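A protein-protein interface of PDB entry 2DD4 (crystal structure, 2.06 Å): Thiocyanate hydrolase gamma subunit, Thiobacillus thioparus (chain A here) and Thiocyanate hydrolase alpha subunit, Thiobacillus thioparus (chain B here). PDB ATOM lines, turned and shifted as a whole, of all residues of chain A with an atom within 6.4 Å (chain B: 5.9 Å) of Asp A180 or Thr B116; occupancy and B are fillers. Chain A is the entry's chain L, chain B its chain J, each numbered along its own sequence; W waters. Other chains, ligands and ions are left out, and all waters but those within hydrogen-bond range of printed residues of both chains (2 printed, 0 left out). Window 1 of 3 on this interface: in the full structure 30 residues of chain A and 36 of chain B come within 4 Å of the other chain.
The side-chain amide nitrogen of Asn A182 sits at hydrogen-bond distance from the side-chain sulfur of Met B57 (3.4 Å).
The side-chain carboxylate (OD2) of Asp A180 lies within hydrogen-bond range of the side-chain hydroxyl (OH) of Tyr B59, at 2.7 Å.
N of Glu B115 is in hydrogen-bond range of O of Val A178, 2.8 Å away.
O of Glu B115 lies within hydrogen-bond range of N of Asp A180, at 2.9 Å.
The side-chain hydroxyl of Thr B116 lies within hydrogen-bond range of the backbone carbonyl oxygen of Asp A180.
OG1 of Thr B116 is in hydrogen-bond range of OD1 of Asn A182, at 2.7 Å.
ND2 of Asn A182 sits at hydrogen-bond distance from O of Glu B117, 2.7 Å away.
O of Glu B117 sits at hydrogen-bond distance from NE2 of Gln A183 (3.4 Å).
The side-chain carboxylate of Glu B117 lies within hydrogen-bond range of the side-chain hydroxyl of Thr A185 (2.5 Å).
The side-chain carboxylate (OE2) of Glu B115 lies within hydrogen-bond range of the side-chain hydroxyl (OG) of Ser B93.
O of Val A125 lies within hydrogen-bond range of N of Ala A179, 2.9 Å away.
The backbone carbonyl oxygen of Ala A179 is in hydrogen-bond range of the backbone NH of Val A127, 3.0 Å away.
The side-chain hydroxyl (OG1) of Thr A129 is in hydrogen-bond range of the side-chain carboxylate (OD2) of Asp A180 (2.7 Å).
O of Asp A180 sits close to OD1 of Asn A182 (3.3 Å).
The side-chain amide nitrogen of Asn A182 lies close to the side-chain amide nitrogen of Gln A183, 3.5 Å away.
Met B57 touches Thr A129 (CG to OG1, 3.5 Å).
Leu A130 touches Met B57 (CD1 to SD, 3.9 Å).
Val A156 touches Tyr B59 (CG1 to OH, 3.7 Å).
CD1 of Leu B114 touches CB of Val A156 (3.7 Å).
CA of Leu B114 touches O of Val A178 (3.3 Å).
O of Glu B115 touches CA of Ala A179 (3.4 Å).
Asp A180 touches Met B57 (OD2 to CE, 3.4 Å).
Asp A180 touches just these residues of chain B: Met B57, Tyr B59, Glu B115 and Thr B116.
Thr B116 touches two residues of chain A.
Printed residues of chain A within 4 Å of Glu B115: Val A178 (2.8 Å), Ala A179 (3.4 Å) and Asp A180 (2.9 Å).
Of the printed residues of chain B, Thr A185 touches Glu B117.
Of the printed residues of chain B, Val A178 touches Leu B114 (3.3 Å) and Glu B115 (2.8 Å).
Of the printed residues of chain A, Leu B114 touches Val A156 (3.7 Å) and Val A178 (3.3 Å).
Printed residues of chain B within 4 Å of Leu A130: Met B57.
Val A125 touches none of the printed residues of chain B.
Val A127 touches none of the printed residues of chain B.
The nearest residue of chain A that does not touch Thr B116 is Tyr A187 (4.8 Å).
The nearest printed residue of chain B that does not touch Thr A129 is Tyr B59 (4.1 Å).
Hydrophobic or aromatic side chains of chain B that line the printed part of chain A: Met B57, Tyr B59 and Leu B114.
Hydrophobic or aromatic side chains of chain A that line the printed part of chain B: Leu A130 and Val A156.
Water W2 lies within hydrogen-bond range of the side-chain hydroxyl (OH) of Tyr A187 (2.7 Å), the side-chain hydroxyl (OG) of Ser B93 (2.8 Å) and the side-chain carboxylate (OE2) of Glu B117 (2.8 Å).
Water W1 lies within hydrogen-bond range of the backbone NH (N) of Gln A183 (2.8 Å), the backbone carbonyl oxygen (O) of Thr A185 (2.9 Å), the backbone NH (N) of Asn A182 (3.4 Å) and the side-chain carboxylate (OE1) of Glu B117 (3.4 Å).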
ATOM      1  N   VAL A 125      -7.050  35.116 -21.318  1.00  0.00           N
ATOM      2  CA  VAL A 125      -6.076  35.450 -22.344  1.00  0.00           C
ATOM      3  C   VAL A 125      -4.953  34.435 -22.144  1.00  0.00           C
ATOM      4  O   VAL A 125      -4.565  34.133 -21.014  1.00  0.00           O
ATOM      5  CB  VAL A 125      -5.561  36.906 -22.242  1.00  0.00           C
ATOM      6  CG1 VAL A 125      -4.824  37.137 -20.932  1.00  0.00           C
ATOM      7  CG2 VAL A 125      -4.676  37.205 -23.445  1.00  0.00           C
ATOM      8  N   VAL A 126      -4.443  33.894 -23.245  1.00  0.00           N
ATOM      9  CA  VAL A 126      -3.430  32.852 -23.169  1.00  0.00           C
ATOM     10  C   VAL A 126      -2.021  33.226 -23.605  1.00  0.00           C
ATOM     11  O   VAL A 126      -1.827  34.039 -24.515  1.00  0.00           O
ATOM     12  CB  VAL A 126      -3.881  31.629 -24.005  1.00  0.00           C
ATOM     13  CG1 VAL A 126      -2.904  30.473 -23.827  1.00  0.00           C
ATOM     14  CG2 VAL A 126      -5.292  31.217 -23.601  1.00  0.00           C
ATOM     15  N   VAL A 127      -1.042  32.602 -22.952  1.00  0.00           N
ATOM     16  CA  VAL A 127       0.367  32.811 -23.262  1.00  0.00           C
ATOM     17  C   VAL A 127       1.171  31.573 -22.849  1.00  0.00           C
ATOM     18  O   VAL A 127       0.680  30.714 -22.113  1.00  0.00           O
ATOM     19  CB  VAL A 127       0.937  34.057 -22.502  1.00  0.00           C
ATOM     20  CG1 VAL A 127       0.913  33.816 -20.993  1.00  0.00           C
ATOM     21  CG2 VAL A 127       2.365  34.360 -22.968  1.00  0.00           C
ATOM     22  N   CYS A 128       2.391  31.464 -23.360  1.00  0.00           N
ATOM     23  CA  CYS A 128       3.292  30.382 -22.978  1.00  0.00           C
ATOM     24  C   CYS A 128       4.592  31.106 -22.686  1.00  0.00           C
ATOM     25  O   CYS A 128       5.358  31.403 -23.601  1.00  0.00           O
ATOM     26  CB  CYS A 128       3.512  29.375 -24.107  1.00  0.00           C
ATOM     27  SG  CYS A 128       4.748  28.105 -23.667  1.00  0.00           S
ATOM     28  N   THR A 129       4.831  31.410 -21.415  1.00  0.00           N
ATOM     29  CA  THR A 129       6.034  32.141 -21.033  1.00  0.00           C
ATOM     30  C   THR A 129       7.329  31.387 -21.309  1.00  0.00           C
ATOM     31  O   THR A 129       8.378  31.999 -21.520  1.00  0.00           O
ATOM     32  CB  THR A 129       5.992  32.538 -19.542  1.00  0.00           C
ATOM     33  OG1 THR A 129       5.963  31.360 -18.724  1.00  0.00           O
ATOM     34  CG2 THR A 129       4.752  33.381 -19.258  1.00  0.00           C
ATOM     35  N   LEU A 130       7.256  30.062 -21.327  1.00  0.00           N
ATOM     36  CA  LEU A 130       8.439  29.238 -21.556  1.00  0.00           C
ATOM     37  C   LEU A 130       8.812  29.083 -23.027  1.00  0.00           C
ATOM     38  O   LEU A 130       9.953  28.750 -23.354  1.00  0.00           O
ATOM     39  CB  LEU A 130       8.235  27.862 -20.912  1.00  0.00           C
ATOM     40  CG  LEU A 130       8.026  27.927 -19.394  1.00  0.00           C
ATOM     41  CD1 LEU A 130       7.771  26.532 -18.832  1.00  0.00           C
ATOM     42  CD2 LEU A 130       9.269  28.554 -18.743  1.00  0.00           C
ATOM     43  N   VAL A 156       1.738  37.853 -18.316  1.00  0.00           N
ATOM     44  CA  VAL A 156       1.426  37.283 -17.007  1.00  0.00           C
ATOM     45  C   VAL A 156       1.437  38.300 -15.872  1.00  0.00           C
ATOM     46  O   VAL A 156       0.744  38.122 -14.869  1.00  0.00           O
ATOM     47  CB  VAL A 156       2.406  36.146 -16.623  1.00  0.00           C
ATOM     48  CG1 VAL A 156       2.215  34.952 -17.552  1.00  0.00           C
ATOM     49  CG2 VAL A 156       3.848  36.650 -16.676  1.00  0.00           C
ATOM     50  N   VAL A 178      -5.118  35.004 -16.776  1.00  0.00           N
ATOM     51  CA  VAL A 178      -4.085  34.704 -17.745  1.00  0.00           C
ATOM     52  C   VAL A 178      -3.771  33.222 -17.605  1.00  0.00           C
ATOM     53  O   VAL A 178      -3.497  32.742 -16.502  1.00  0.00           O
ATOM     54  CB  VAL A 178      -2.792  35.505 -17.475  1.00  0.00           C
ATOM     55  CG1 VAL A 178      -1.722  35.093 -18.470  1.00  0.00           C
ATOM     56  CG2 VAL A 178      -3.067  37.006 -17.569  1.00  0.00           C
ATOM     57  N   ALA A 179      -3.835  32.496 -18.714  1.00  0.00           N
ATOM     58  CA  ALA A 179      -3.522  31.072 -18.699  1.00  0.00           C
ATOM     59  C   ALA A 179      -2.134  30.901 -19.302  1.00  0.00           C
ATOM     60  O   ALA A 179      -1.900  31.281 -20.448  1.00  0.00           O
ATOM     61  CB  ALA A 179      -4.544  30.288 -19.513  1.00  0.00           C
ATOM     62  N   ASP A 180      -1.213  30.347 -18.521  1.00  0.00           N
ATOM     63  CA  ASP A 180       0.150  30.117 -18.997  1.00  0.00           C
ATOM     64  C   ASP A 180       0.246  28.632 -19.327  1.00  0.00           C
ATOM     65  O   ASP A 180       0.280  27.798 -18.423  1.00  0.00           O
ATOM     66  CB  ASP A 180       1.162  30.484 -17.899  1.00  0.00           C
ATOM     67  CG  ASP A 180       2.604  30.493 -18.397  1.00  0.00           C
ATOM     68  OD1 ASP A 180       2.852  30.080 -19.549  1.00  0.00           O
ATOM     69  OD2 ASP A 180       3.496  30.914 -17.626  1.00  0.00           O
ATOM     70  N   SER A 181       0.266  28.297 -20.615  1.00  0.00           N
ATOM     71  CA  SER A 181       0.348  26.894 -21.025  1.00  0.00           C
ATOM     72  C   SER A 181       1.795  26.437 -20.974  1.00  0.00           C
ATOM     73  O   SER A 181       2.494  26.424 -21.983  1.00  0.00           O
ATOM     74  CB  SER A 181      -0.231  26.705 -22.433  1.00  0.00           C
ATOM     75  OG  SER A 181       0.024  27.830 -23.246  1.00  0.00           O
ATOM     76  N   ASN A 182       2.221  26.047 -19.777  1.00  0.00           N
ATOM     77  CA  ASN A 182       3.593  25.625 -19.526  1.00  0.00           C
ATOM     78  C   ASN A 182       3.841  24.120 -19.540  1.00  0.00           C
ATOM     79  O   ASN A 182       4.991  23.690 -19.458  1.00  0.00           O
ATOM     80  CB  ASN A 182       4.040  26.189 -18.181  1.00  0.00           C
ATOM     81  CG  ASN A 182       3.247  25.609 -17.028  1.00  0.00           C
ATOM     82  OD1 ASN A 182       2.047  25.359 -17.153  1.00  0.00           O
ATOM     83  ND2 ASN A 182       3.909  25.399 -15.896  1.00  0.00           N
ATOM     84  N   GLN A 183       2.784  23.315 -19.617  1.00  0.00           N
ATOM     85  CA  GLN A 183       2.968  21.869 -19.647  1.00  0.00           C
ATOM     86  C   GLN A 183       2.337  21.287 -20.915  1.00  0.00           C
ATOM     87  O   GLN A 183       2.499  21.851 -21.995  1.00  0.00           O
ATOM     88  CB  GLN A 183       2.381  21.214 -18.384  1.00  0.00           C
ATOM     89  CG  GLN A 183       2.923  21.758 -17.048  1.00  0.00           C
ATOM     90  CD  GLN A 183       4.412  21.474 -16.798  1.00  0.00           C
ATOM     91  OE1 GLN A 183       5.051  20.708 -17.518  1.00  0.00           O
ATOM     92  NE2 GLN A 183       4.960  22.093 -15.758  1.00  0.00           N
ATOM     93  N   THR A 185      -0.994  20.903 -21.601  1.00  0.00           N
ATOM     94  CA  THR A 185      -2.310  21.426 -21.948  1.00  0.00           C
ATOM     95  C   THR A 185      -2.193  22.617 -22.906  1.00  0.00           C
ATOM     96  O   THR A 185      -1.285  23.444 -22.782  1.00  0.00           O
ATOM     97  CB  THR A 185      -3.089  21.880 -20.685  1.00  0.00           C
ATOM     98  OG1 THR A 185      -3.571  20.730 -19.977  1.00  0.00           O
ATOM     99  CG2 THR A 185      -4.273  22.759 -21.065  1.00  0.00           C
ATOM    100  N   TYR A 187      -4.704  25.672 -24.776  1.00  0.00           N
ATOM    101  CA  TYR A 187      -5.995  26.332 -24.577  1.00  0.00           C
ATOM    102  C   TYR A 187      -6.510  27.137 -25.769  1.00  0.00           C
ATOM    103  O   TYR A 187      -5.740  27.571 -26.625  1.00  0.00           O
ATOM    104  CB  TYR A 187      -5.913  27.357 -23.434  1.00  0.00           C
ATOM    105  CG  TYR A 187      -5.322  26.898 -22.124  1.00  0.00           C
ATOM    106  CD1 TYR A 187      -6.092  26.209 -21.190  1.00  0.00           C
ATOM    107  CD2 TYR A 187      -3.998  27.199 -21.796  1.00  0.00           C
ATOM    108  CE1 TYR A 187      -5.564  25.835 -19.960  1.00  0.00           C
ATOM    109  CE2 TYR A 187      -3.457  26.827 -20.563  1.00  0.00           C
ATOM    110  CZ  TYR A 187      -4.247  26.147 -19.651  1.00  0.00           C
ATOM    111  OH  TYR A 187      -3.728  25.777 -18.432  1.00  0.00           O
ATOM    112  N   MET B  57       7.751  27.775 -13.689  1.00  0.00           N
ATOM    113  CA  MET B  57       8.290  29.129 -13.744  1.00  0.00           C
ATOM    114  C   MET B  57       8.764  29.707 -12.422  1.00  0.00           C
ATOM    115  O   MET B  57       8.163  29.481 -11.370  1.00  0.00           O
ATOM    116  CB  MET B  57       7.269  30.085 -14.370  1.00  0.00           C
ATOM    117  CG  MET B  57       6.849  29.738 -15.799  1.00  0.00           C
ATOM    118  SD  MET B  57       5.788  28.284 -15.905  1.00  0.00           S
ATOM    119  CE  MET B  57       4.321  28.880 -14.988  1.00  0.00           C
ATOM    120  N   TYR B  59       8.557  32.685 -11.435  1.00  0.00           N
ATOM    121  CA  TYR B  59       7.587  33.605 -10.855  1.00  0.00           C
ATOM    122  C   TYR B  59       6.545  32.961  -9.942  1.00  0.00           C
ATOM    123  O   TYR B  59       5.814  33.668  -9.247  1.00  0.00           O
ATOM    124  CB  TYR B  59       6.902  34.443 -11.959  1.00  0.00           C
ATOM    125  CG  TYR B  59       5.852  33.748 -12.815  1.00  0.00           C
ATOM    126  CD1 TYR B  59       4.575  33.481 -12.318  1.00  0.00           C
ATOM    127  CD2 TYR B  59       6.116  33.426 -14.150  1.00  0.00           C
ATOM    128  CE1 TYR B  59       3.578  32.917 -13.132  1.00  0.00           C
ATOM    129  CE2 TYR B  59       5.134  32.862 -14.971  1.00  0.00           C
ATOM    130  CZ  TYR B  59       3.866  32.613 -14.457  1.00  0.00           C
ATOM    131  OH  TYR B  59       2.886  32.083 -15.275  1.00  0.00           O
ATOM    132  N   THR B  60       6.486  31.630  -9.921  1.00  0.00           N
ATOM    133  CA  THR B  60       5.523  30.928  -9.072  1.00  0.00           C
ATOM    134  C   THR B  60       6.111  30.392  -7.767  1.00  0.00           C
ATOM    135  O   THR B  60       5.365  30.018  -6.865  1.00  0.00           O
ATOM    136  CB  THR B  60       4.900  29.704  -9.783  1.00  0.00           C
ATOM    137  OG1 THR B  60       5.926  28.736 -10.043  1.00  0.00           O
ATOM    138  CG2 THR B  60       4.225  30.109 -11.088  1.00  0.00           C
ATOM    139  N   TYR B  92      -1.423  19.257 -11.931  1.00  0.00           N
ATOM    140  CA  TYR B  92      -2.558  20.016 -11.431  1.00  0.00           C
ATOM    141  C   TYR B  92      -2.609  21.401 -12.042  1.00  0.00           C
ATOM    142  O   TYR B  92      -1.573  22.022 -12.277  1.00  0.00           O
ATOM    143  CB  TYR B  92      -2.450  20.177  -9.913  1.00  0.00           C
ATOM    144  CG  TYR B  92      -2.342  18.888  -9.129  1.00  0.00           C
ATOM    145  CD1 TYR B  92      -3.460  18.332  -8.503  1.00  0.00           C
ATOM    146  CD2 TYR B  92      -1.115  18.240  -8.984  1.00  0.00           C
ATOM    147  CE1 TYR B  92      -3.357  17.161  -7.747  1.00  0.00           C
ATOM    148  CE2 TYR B  92      -1.000  17.070  -8.234  1.00  0.00           C
ATOM    149  CZ  TYR B  92      -2.122  16.537  -7.616  1.00  0.00           C
ATOM    150  OH  TYR B  92      -2.007  15.388  -6.864  1.00  0.00           O
ATOM    151  N   SER B  93      -3.814  21.892 -12.300  1.00  0.00           N
ATOM    152  CA  SER B  93      -3.941  23.242 -12.816  1.00  0.00           C
ATOM    153  C   SER B  93      -4.204  24.068 -11.562  1.00  0.00           C
ATOM    154  O   SER B  93      -5.157  23.801 -10.824  1.00  0.00           O
ATOM    155  CB  SER B  93      -5.107  23.361 -13.791  1.00  0.00           C
ATOM    156  OG  SER B  93      -5.008  24.580 -14.509  1.00  0.00           O
ATOM    157  N   ILE B  94      -3.346  25.051 -11.308  1.00  0.00           N
ATOM    158  CA  ILE B  94      -3.472  25.887 -10.123  1.00  0.00           C
ATOM    159  C   ILE B  94      -3.775  27.336 -10.464  1.00  0.00           C
ATOM    160  O   ILE B  94      -3.223  27.892 -11.415  1.00  0.00           O
ATOM    161  CB  ILE B  94      -2.174  25.843  -9.269  1.00  0.00           C
ATOM    162  CG1 ILE B  94      -1.980  24.446  -8.669  1.00  0.00           C
ATOM    163  CG2 ILE B  94      -2.252  26.854  -8.134  1.00  0.00           C
ATOM    164  CD1 ILE B  94      -1.520  23.424  -9.638  1.00  0.00           C
ATOM    165  N   VAL B  95      -4.655  27.943  -9.674  1.00  0.00           N
ATOM    166  CA  VAL B  95      -5.027  29.338  -9.869  1.00  0.00           C
ATOM    167  C   VAL B  95      -4.407  30.208  -8.777  1.00  0.00           C
ATOM    168  O   VAL B  95      -4.560  29.934  -7.583  1.00  0.00           O
ATOM    169  CB  VAL B  95      -6.559  29.515  -9.850  1.00  0.00           C
ATOM    170  CG1 VAL B  95      -6.921  31.001  -9.832  1.00  0.00           C
ATOM    171  CG2 VAL B  95      -7.169  28.839 -11.080  1.00  0.00           C
ATOM    172  N   PHE B  96      -3.704  31.254  -9.200  1.00  0.00           N
ATOM    173  CA  PHE B  96      -3.050  32.186  -8.288  1.00  0.00           C
ATOM    174  C   PHE B  96      -3.707  33.555  -8.380  1.00  0.00           C
ATOM    175  O   PHE B  96      -4.120  33.982  -9.461  1.00  0.00           O
ATOM    176  CB  PHE B  96      -1.578  32.367  -8.671  1.00  0.00           C
ATOM    177  CG  PHE B  96      -0.746  31.119  -8.557  1.00  0.00           C
ATOM    178  CD1 PHE B  96      -0.202  30.738  -7.332  1.00  0.00           C
ATOM    179  CD2 PHE B  96      -0.463  30.353  -9.684  1.00  0.00           C
ATOM    180  CE1 PHE B  96       0.618  29.614  -7.233  1.00  0.00           C
ATOM    181  CE2 PHE B  96       0.354  29.228  -9.597  1.00  0.00           C
ATOM    182  CZ  PHE B  96       0.897  28.858  -8.368  1.00  0.00           C
ATOM    183  N   LEU B 114      -4.127  34.060 -12.334  1.00  0.00           N
ATOM    184  CA  LEU B 114      -3.228  33.415 -13.282  1.00  0.00           C
ATOM    185  C   LEU B 114      -3.362  31.908 -13.067  1.00  0.00           C
ATOM    186  O   LEU B 114      -3.268  31.432 -11.934  1.00  0.00           O
ATOM    187  CB  LEU B 114      -1.780  33.868 -13.041  1.00  0.00           C
ATOM    188  CG  LEU B 114      -0.700  33.324 -13.988  1.00  0.00           C
ATOM    189  CD1 LEU B 114       0.451  34.312 -14.067  1.00  0.00           C
ATOM    190  CD2 LEU B 114      -0.208  31.961 -13.510  1.00  0.00           C
ATOM    191  N   GLU B 115      -3.606  31.167 -14.145  1.00  0.00           N
ATOM    192  CA  GLU B 115      -3.750  29.716 -14.057  1.00  0.00           C
ATOM    193  C   GLU B 115      -2.640  29.041 -14.851  1.00  0.00           C
ATOM    194  O   GLU B 115      -2.361  29.419 -15.991  1.00  0.00           O
ATOM    195  CB  GLU B 115      -5.118  29.269 -14.603  1.00  0.00           C
ATOM    196  CG  GLU B 115      -5.463  27.813 -14.264  1.00  0.00           C
ATOM    197  CD  GLU B 115      -6.815  27.362 -14.794  1.00  0.00           C
ATOM    198  OE1 GLU B 115      -7.697  28.220 -15.015  1.00  0.00           O
ATOM    199  OE2 GLU B 115      -7.006  26.136 -14.969  1.00  0.00           O
ATOM    200  N   THR B 116      -1.994  28.052 -14.244  1.00  0.00           N
ATOM    201  CA  THR B 116      -0.919  27.331 -14.918  1.00  0.00           C
ATOM    202  C   THR B 116      -0.814  25.926 -14.319  1.00  0.00           C
ATOM    203  O   THR B 116      -1.391  25.657 -13.264  1.00  0.00           O
ATOM    204  CB  THR B 116       0.427  28.107 -14.801  1.00  0.00           C
ATOM    205  OG1 THR B 116       1.372  27.579 -15.741  1.00  0.00           O
ATOM    206  CG2 THR B 116       0.995  27.999 -13.395  1.00  0.00           C
ATOM    207  N   GLU B 117      -0.093  25.032 -14.989  1.00  0.00           N
ATOM    208  CA  GLU B 117       0.024  23.655 -14.519  1.00  0.00           C
ATOM    209  C   GLU B 117       1.351  23.328 -13.848  1.00  0.00           C
ATOM    210  O   GLU B 117       2.414  23.740 -14.307  1.00  0.00           O
ATOM    211  CB  GLU B 117      -0.235  22.688 -15.683  1.00  0.00           C
ATOM    212  CG  GLU B 117      -1.595  22.913 -16.344  1.00  0.00           C
ATOM    213  CD  GLU B 117      -1.949  21.860 -17.382  1.00  0.00           C
ATOM    214  OE1 GLU B 117      -1.030  21.191 -17.910  1.00  0.00           O
ATOM    215  OE2 GLU B 117      -3.155  21.717 -17.683  1.00  0.00           O
ATOM    216  N   ILE B 118       1.270  22.565 -12.761  1.00  0.00           N
ATOM    217  CA  ILE B 118       2.440  22.182 -11.979  1.00  0.00           C
ATOM    218  C   ILE B 118       2.375  20.707 -11.579  1.00  0.00           C
ATOM    219  O   ILE B 118       1.345  20.236 -11.090  1.00  0.00           O
ATOM    220  CB  ILE B 118       2.517  23.018 -10.679  1.00  0.00           C
ATOM    221  CG1 ILE B 118       2.498  24.514 -11.007  1.00  0.00           C
ATOM    222  CG2 ILE B 118       3.774  22.663  -9.903  1.00  0.00           C
ATOM    223  CD1 ILE B 118       3.678  24.976 -11.803  1.00  0.00           C
HETATM  224  O   HOH W   1       0.065  23.433 -20.254  1.00  0.00           O
HETATM  225  O   HOH W   2      -4.932  23.761 -17.144  1.00  0.00           O
